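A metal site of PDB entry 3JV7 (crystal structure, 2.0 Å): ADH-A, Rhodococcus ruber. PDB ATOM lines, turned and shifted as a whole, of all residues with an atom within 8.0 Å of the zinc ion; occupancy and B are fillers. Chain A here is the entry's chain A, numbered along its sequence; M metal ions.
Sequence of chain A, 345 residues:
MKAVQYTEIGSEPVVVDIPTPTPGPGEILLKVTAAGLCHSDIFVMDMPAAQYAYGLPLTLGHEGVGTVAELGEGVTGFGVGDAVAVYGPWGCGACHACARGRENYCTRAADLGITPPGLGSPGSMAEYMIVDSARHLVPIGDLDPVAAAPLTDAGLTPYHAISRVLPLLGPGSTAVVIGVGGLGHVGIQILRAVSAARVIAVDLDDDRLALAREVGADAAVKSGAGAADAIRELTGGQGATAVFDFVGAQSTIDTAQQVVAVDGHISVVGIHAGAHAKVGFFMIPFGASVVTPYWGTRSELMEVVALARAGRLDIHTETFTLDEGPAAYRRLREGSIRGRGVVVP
The side-chain sulfur of Cys 95 lies close to the backbone NH of Thr 107. N of Ala 97 sits close to SG of Cys 95. The backbone NH of Gly 93 lies close to the side-chain sulfur of Cys 98 (3.2 Å). N of Arg 108 lies close to SG of Cys 106, 3.3 Å away. SG of Cys 106 lies close to N of Ala 109 (3.3 Å). The side-chain sulfur of Cys 92 sits close to the backbone NH of Ala 94 (3.4 Å).
N of Gly 93 touches the zinc ion (3.8 Å). Five residues have an atom within 4 Å of the zinc ion: Cys 92, Gly 93, Cys 95, Cys 98 and Cys 106. The nearest printed residue that does not touch the zinc ion is Thr 107 (4.2 Å).
SG of Cys 95 is bound to the zinc ion (2.3 Å). The zinc ion is bound by the side-chain sulfur (SG) of Cys 98 (2.3 Å). SG of Cys 106 binds the zinc ion. The side-chain sulfur (SG) of Cys 92 binds the zinc ion (2.4 Å). The zinc ion has four donor atoms within binding distance.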
ATOM      1  N   TRP A  90     -24.131 -16.096  19.045  1.00  0.00           N
ATOM      2  CA  TRP A  90     -23.965 -15.895  17.598  1.00  0.00           C
ATOM      3  C   TRP A  90     -22.695 -16.546  17.059  1.00  0.00           C
ATOM      4  O   TRP A  90     -21.641 -16.433  17.678  1.00  0.00           O
ATOM      5  CB  TRP A  90     -23.936 -14.406  17.270  1.00  0.00           C
ATOM      6  CG  TRP A  90     -25.200 -13.695  17.624  1.00  0.00           C
ATOM      7  CD1 TRP A  90     -26.373 -14.267  18.041  1.00  0.00           C
ATOM      8  CD2 TRP A  90     -25.425 -12.285  17.593  1.00  0.00           C
ATOM      9  NE1 TRP A  90     -27.307 -13.289  18.290  1.00  0.00           N
ATOM     10  CE2 TRP A  90     -26.759 -12.062  18.010  1.00  0.00           C
ATOM     11  CE3 TRP A  90     -24.627 -11.187  17.252  1.00  0.00           C
ATOM     12  CZ2 TRP A  90     -27.309 -10.784  18.091  1.00  0.00           C
ATOM     13  CZ3 TRP A  90     -25.177  -9.908  17.332  1.00  0.00           C
ATOM     14  CH2 TRP A  90     -26.515  -9.726  17.763  1.00  0.00           C
ATOM     15  N   GLY A  91     -22.816 -17.204  15.913  1.00  0.00           N
ATOM     16  CA  GLY A  91     -21.685 -17.876  15.286  1.00  0.00           C
ATOM     17  C   GLY A  91     -21.473 -17.392  13.855  1.00  0.00           C
ATOM     18  O   GLY A  91     -22.178 -16.501  13.402  1.00  0.00           O
ATOM     19  N   CYS A  92     -20.523 -17.969  13.118  1.00  0.00           N
ATOM     20  CA  CYS A  92     -20.236 -17.440  11.776  1.00  0.00           C
ATOM     21  C   CYS A  92     -21.341 -17.845  10.794  1.00  0.00           C
ATOM     22  O   CYS A  92     -21.577 -17.162   9.806  1.00  0.00           O
ATOM     23  CB  CYS A  92     -18.856 -17.875  11.272  1.00  0.00           C
ATOM     24  SG  CYS A  92     -18.691 -19.659  10.937  1.00  0.00           S
ATOM     25  N   GLY A  93     -22.026 -18.947  11.089  1.00  0.00           N
ATOM     26  CA  GLY A  93     -23.097 -19.406  10.228  1.00  0.00           C
ATOM     27  C   GLY A  93     -22.630 -20.283   9.078  1.00  0.00           C
ATOM     28  O   GLY A  93     -23.463 -20.835   8.351  1.00  0.00           O
ATOM     29  N   ALA A  94     -21.312 -20.459   8.939  1.00  0.00           N
ATOM     30  CA  ALA A  94     -20.759 -21.177   7.778  1.00  0.00           C
ATOM     31  C   ALA A  94     -19.870 -22.392   8.096  1.00  0.00           C
ATOM     32  O   ALA A  94     -19.639 -23.220   7.206  1.00  0.00           O
ATOM     33  CB  ALA A  94     -19.996 -20.193   6.865  1.00  0.00           C
ATOM     34  N   CYS A  95     -19.347 -22.490   9.322  1.00  0.00           N
ATOM     35  CA  CYS A  95     -18.473 -23.606   9.686  1.00  0.00           C
ATOM     36  C   CYS A  95     -19.284 -24.878   9.880  1.00  0.00           C
ATOM     37  O   CYS A  95     -20.522 -24.846   9.924  1.00  0.00           O
ATOM     38  CB  CYS A  95     -17.673 -23.278  10.955  1.00  0.00           C
ATOM     39  SG  CYS A  95     -18.628 -23.252  12.480  1.00  0.00           S
ATOM     40  N   HIS A  96     -18.585 -26.011   9.996  1.00  0.00           N
ATOM     41  CA  HIS A  96     -19.229 -27.321  10.197  1.00  0.00           C
ATOM     42  C   HIS A  96     -20.187 -27.323  11.400  1.00  0.00           C
ATOM     43  O   HIS A  96     -21.307 -27.830  11.319  1.00  0.00           O
ATOM     44  CB  HIS A  96     -18.160 -28.410  10.360  1.00  0.00           C
ATOM     45  CG  HIS A  96     -18.699 -29.802  10.270  1.00  0.00           C
ATOM     46  ND1 HIS A  96     -19.022 -30.550  11.386  1.00  0.00           N
ATOM     47  CD2 HIS A  96     -18.975 -30.591   9.201  1.00  0.00           C
ATOM     48  CE1 HIS A  96     -19.465 -31.733  11.004  1.00  0.00           C
ATOM     49  NE2 HIS A  96     -19.456 -31.781   9.684  1.00  0.00           N
ATOM     50  N   ALA A  97     -19.733 -26.766  12.528  1.00  0.00           N
ATOM     51  CA  ALA A  97     -20.587 -26.631  13.704  1.00  0.00           C
ATOM     52  C   ALA A  97     -21.822 -25.765  13.421  1.00  0.00           C
ATOM     53  O   ALA A  97     -22.954 -26.170  13.718  1.00  0.00           O
ATOM     54  CB  ALA A  97     -19.776 -26.057  14.908  1.00  0.00           C
ATOM     55  N   CYS A  98     -21.614 -24.588  12.857  1.00  0.00           N
ATOM     56  CA  CYS A  98     -22.741 -23.697  12.569  1.00  0.00           C
ATOM     57  C   CYS A  98     -23.716 -24.326  11.580  1.00  0.00           C
ATOM     58  O   CYS A  98     -24.944 -24.173  11.702  1.00  0.00           O
ATOM     59  CB  CYS A  98     -22.270 -22.310  12.066  1.00  0.00           C
ATOM     60  SG  CYS A  98     -21.507 -21.223  13.314  1.00  0.00           S
ATOM     61  N   ALA A  99     -23.178 -25.057  10.605  1.00  0.00           N
ATOM     62  CA  ALA A  99     -24.020 -25.700   9.594  1.00  0.00           C
ATOM     63  C   ALA A  99     -25.007 -26.698  10.207  1.00  0.00           C
ATOM     64  O   ALA A  99     -26.015 -27.054   9.591  1.00  0.00           O
ATOM     65  CB  ALA A  99     -23.160 -26.372   8.536  1.00  0.00           C
ATOM     66  N   ARG A 102     -25.333 -25.528  15.578  1.00  0.00           N
ATOM     67  CA  ARG A 102     -24.582 -25.511  16.840  1.00  0.00           C
ATOM     68  C   ARG A 102     -23.656 -24.323  16.907  1.00  0.00           C
ATOM     69  O   ARG A 102     -22.434 -24.462  17.058  1.00  0.00           O
ATOM     70  CB  ARG A 102     -23.784 -26.816  17.013  1.00  0.00           C
ATOM     71  CG  ARG A 102     -24.658 -28.051  16.974  1.00  0.00           C
ATOM     72  CD  ARG A 102     -23.863 -29.347  16.899  1.00  0.00           C
ATOM     73  NE  ARG A 102     -23.179 -29.664  18.147  1.00  0.00           N
ATOM     74  CZ  ARG A 102     -23.752 -30.227  19.195  1.00  0.00           C
ATOM     75  NH1 ARG A 102     -25.036 -30.540  19.175  1.00  0.00           N
ATOM     76  NH2 ARG A 102     -23.047 -30.465  20.280  1.00  0.00           N
ATOM     77  N   GLU A 103     -24.242 -23.133  16.794  1.00  0.00           N
ATOM     78  CA  GLU A 103     -23.451 -21.908  16.705  1.00  0.00           C
ATOM     79  C   GLU A 103     -22.731 -21.625  18.016  1.00  0.00           C
ATOM     80  O   GLU A 103     -21.749 -20.892  18.038  1.00  0.00           O
ATOM     81  CB  GLU A 103     -24.321 -20.718  16.269  1.00  0.00           C
ATOM     82  CG  GLU A 103     -25.006 -20.967  14.934  1.00  0.00           C
ATOM     83  CD  GLU A 103     -25.398 -19.685  14.201  1.00  0.00           C
ATOM     84  OE1 GLU A 103     -25.042 -18.580  14.661  1.00  0.00           O
ATOM     85  OE2 GLU A 103     -26.049 -19.809  13.148  1.00  0.00           O
ATOM     86  N   ASN A 104     -23.235 -22.214  19.102  1.00  0.00           N
ATOM     87  CA  ASN A 104     -22.554 -22.077  20.391  1.00  0.00           C
ATOM     88  C   ASN A 104     -21.162 -22.701  20.341  1.00  0.00           C
ATOM     89  O   ASN A 104     -20.273 -22.321  21.109  1.00  0.00           O
ATOM     90  CB  ASN A 104     -23.407 -22.680  21.527  1.00  0.00           C
ATOM     91  CG  ASN A 104     -23.835 -24.119  21.257  1.00  0.00           C
ATOM     92  OD1 ASN A 104     -24.067 -24.526  20.112  1.00  0.00           O
ATOM     93  ND2 ASN A 104     -23.947 -24.919  22.327  1.00  0.00           N
ATOM     94  N   TYR A 105     -20.976 -23.647  19.441  1.00  0.00           N
ATOM     95  CA  TYR A 105     -19.685 -24.327  19.282  1.00  0.00           C
ATOM     96  C   TYR A 105     -18.977 -23.910  17.986  1.00  0.00           C
ATOM     97  O   TYR A 105     -18.104 -24.603  17.491  1.00  0.00           O
ATOM     98  CB  TYR A 105     -19.867 -25.851  19.362  1.00  0.00           C
ATOM     99  CG  TYR A 105     -20.369 -26.300  20.719  1.00  0.00           C
ATOM    100  CD1 TYR A 105     -19.773 -25.811  21.888  1.00  0.00           C
ATOM    101  CD2 TYR A 105     -21.415 -27.193  20.851  1.00  0.00           C
ATOM    102  CE1 TYR A 105     -20.219 -26.189  23.137  1.00  0.00           C
ATOM    103  CE2 TYR A 105     -21.870 -27.595  22.115  1.00  0.00           C
ATOM    104  CZ  TYR A 105     -21.261 -27.090  23.246  1.00  0.00           C
ATOM    105  OH  TYR A 105     -21.700 -27.460  24.498  1.00  0.00           O
ATOM    106  N   CYS A 106     -19.365 -22.755  17.462  1.00  0.00           N
ATOM    107  CA  CYS A 106     -18.705 -22.174  16.286  1.00  0.00           C
ATOM    108  C   CYS A 106     -17.194 -22.072  16.466  1.00  0.00           C
ATOM    109  O   CYS A 106     -16.704 -21.611  17.493  1.00  0.00           O
ATOM    110  CB  CYS A 106     -19.276 -20.784  16.011  1.00  0.00           C
ATOM    111  SG  CYS A 106     -18.456 -19.951  14.652  1.00  0.00           S
ATOM    112  N   THR A 107     -16.442 -22.510  15.451  1.00  0.00           N
ATOM    113  CA  THR A 107     -14.990 -22.511  15.569  1.00  0.00           C
ATOM    114  C   THR A 107     -14.361 -21.246  14.997  1.00  0.00           C
ATOM    115  O   THR A 107     -13.139 -21.049  15.077  1.00  0.00           O
ATOM    116  CB  THR A 107     -14.381 -23.747  14.856  1.00  0.00           C
ATOM    117  OG1 THR A 107     -15.027 -23.919  13.588  1.00  0.00           O
ATOM    118  CG2 THR A 107     -14.580 -25.020  15.681  1.00  0.00           C
ATOM    119  N   ARG A 108     -15.174 -20.386  14.415  1.00  0.00           N
ATOM    120  CA  ARG A 108     -14.680 -19.161  13.766  1.00  0.00           C
ATOM    121  C   ARG A 108     -15.014 -17.877  14.532  1.00  0.00           C
ATOM    122  O   ARG A 108     -14.381 -16.840  14.317  1.00  0.00           O
ATOM    123  CB  ARG A 108     -15.253 -19.066  12.354  1.00  0.00           C
ATOM    124  CG  ARG A 108     -14.818 -20.211  11.451  1.00  0.00           C
ATOM    125  CD  ARG A 108     -13.419 -20.001  10.914  1.00  0.00           C
ATOM    126  NE  ARG A 108     -13.373 -18.912   9.935  1.00  0.00           N
ATOM    127  CZ  ARG A 108     -12.586 -17.836  10.028  1.00  0.00           C
ATOM    128  NH1 ARG A 108     -12.611 -16.909   9.076  1.00  0.00           N
ATOM    129  NH2 ARG A 108     -11.772 -17.698  11.062  1.00  0.00           N
ATOM    130  N   ALA A 109     -15.995 -17.944  15.439  1.00  0.00           N
ATOM    131  CA  ALA A 109     -16.518 -16.737  16.088  1.00  0.00           C
ATOM    132  C   ALA A 109     -15.432 -15.956  16.842  1.00  0.00           C
ATOM    133  O   ALA A 109     -15.382 -14.724  16.766  1.00  0.00           O
ATOM    134  CB  ALA A 109     -17.677 -17.072  17.033  1.00  0.00           C
ATOM    135  N   LEU A 112     -13.233 -14.154  14.401  1.00  0.00           N
ATOM    136  CA  LEU A 112     -13.962 -13.116  13.681  1.00  0.00           C
ATOM    137  C   LEU A 112     -14.515 -12.011  14.583  1.00  0.00           C
ATOM    138  O   LEU A 112     -15.138 -11.071  14.104  1.00  0.00           O
ATOM    139  CB  LEU A 112     -15.103 -13.738  12.847  1.00  0.00           C
ATOM    140  CG  LEU A 112     -14.716 -14.708  11.729  1.00  0.00           C
ATOM    141  CD1 LEU A 112     -15.973 -15.334  11.122  1.00  0.00           C
ATOM    142  CD2 LEU A 112     -13.889 -13.998  10.640  1.00  0.00           C
ATOM    143  N   ILE A 114     -17.004 -12.254  16.696  1.00  0.00           N
ATOM    144  CA  ILE A 114     -18.451 -12.346  16.728  1.00  0.00           C
ATOM    145  C   ILE A 114     -18.872 -12.650  18.165  1.00  0.00           C
ATOM    146  O   ILE A 114     -18.625 -13.745  18.668  1.00  0.00           O
ATOM    147  CB  ILE A 114     -18.971 -13.463  15.789  1.00  0.00           C
ATOM    148  CG1 ILE A 114     -18.603 -13.137  14.332  1.00  0.00           C
ATOM    149  CG2 ILE A 114     -20.466 -13.626  15.908  1.00  0.00           C
ATOM    150  CD1 ILE A 114     -19.110 -14.168  13.339  1.00  0.00           C
ATOM    151  N   ARG A 135     -31.600 -15.320  11.196  1.00  0.00           N
ATOM    152  CA  ARG A 135     -31.419 -16.664  11.739  1.00  0.00           C
ATOM    153  C   ARG A 135     -31.206 -16.656  13.260  1.00  0.00           C
ATOM    154  O   ARG A 135     -31.243 -17.711  13.889  1.00  0.00           O
ATOM    155  CB  ARG A 135     -30.311 -17.441  11.013  1.00  0.00           C
ATOM    156  CG  ARG A 135     -28.902 -17.169  11.524  1.00  0.00           C
ATOM    157  CD  ARG A 135     -27.843 -18.024  10.794  1.00  0.00           C
ATOM    158  NE  ARG A 135     -26.530 -17.840  11.395  1.00  0.00           N
ATOM    159  CZ  ARG A 135     -25.703 -16.842  11.097  1.00  0.00           C
ATOM    160  NH1 ARG A 135     -26.052 -15.955  10.173  1.00  0.00           N
ATOM    161  NH2 ARG A 135     -24.530 -16.737  11.707  1.00  0.00           N
HETATM  162 ZN    ZN M   1     -19.277 -21.067  12.742  1.00  0.00          ZN
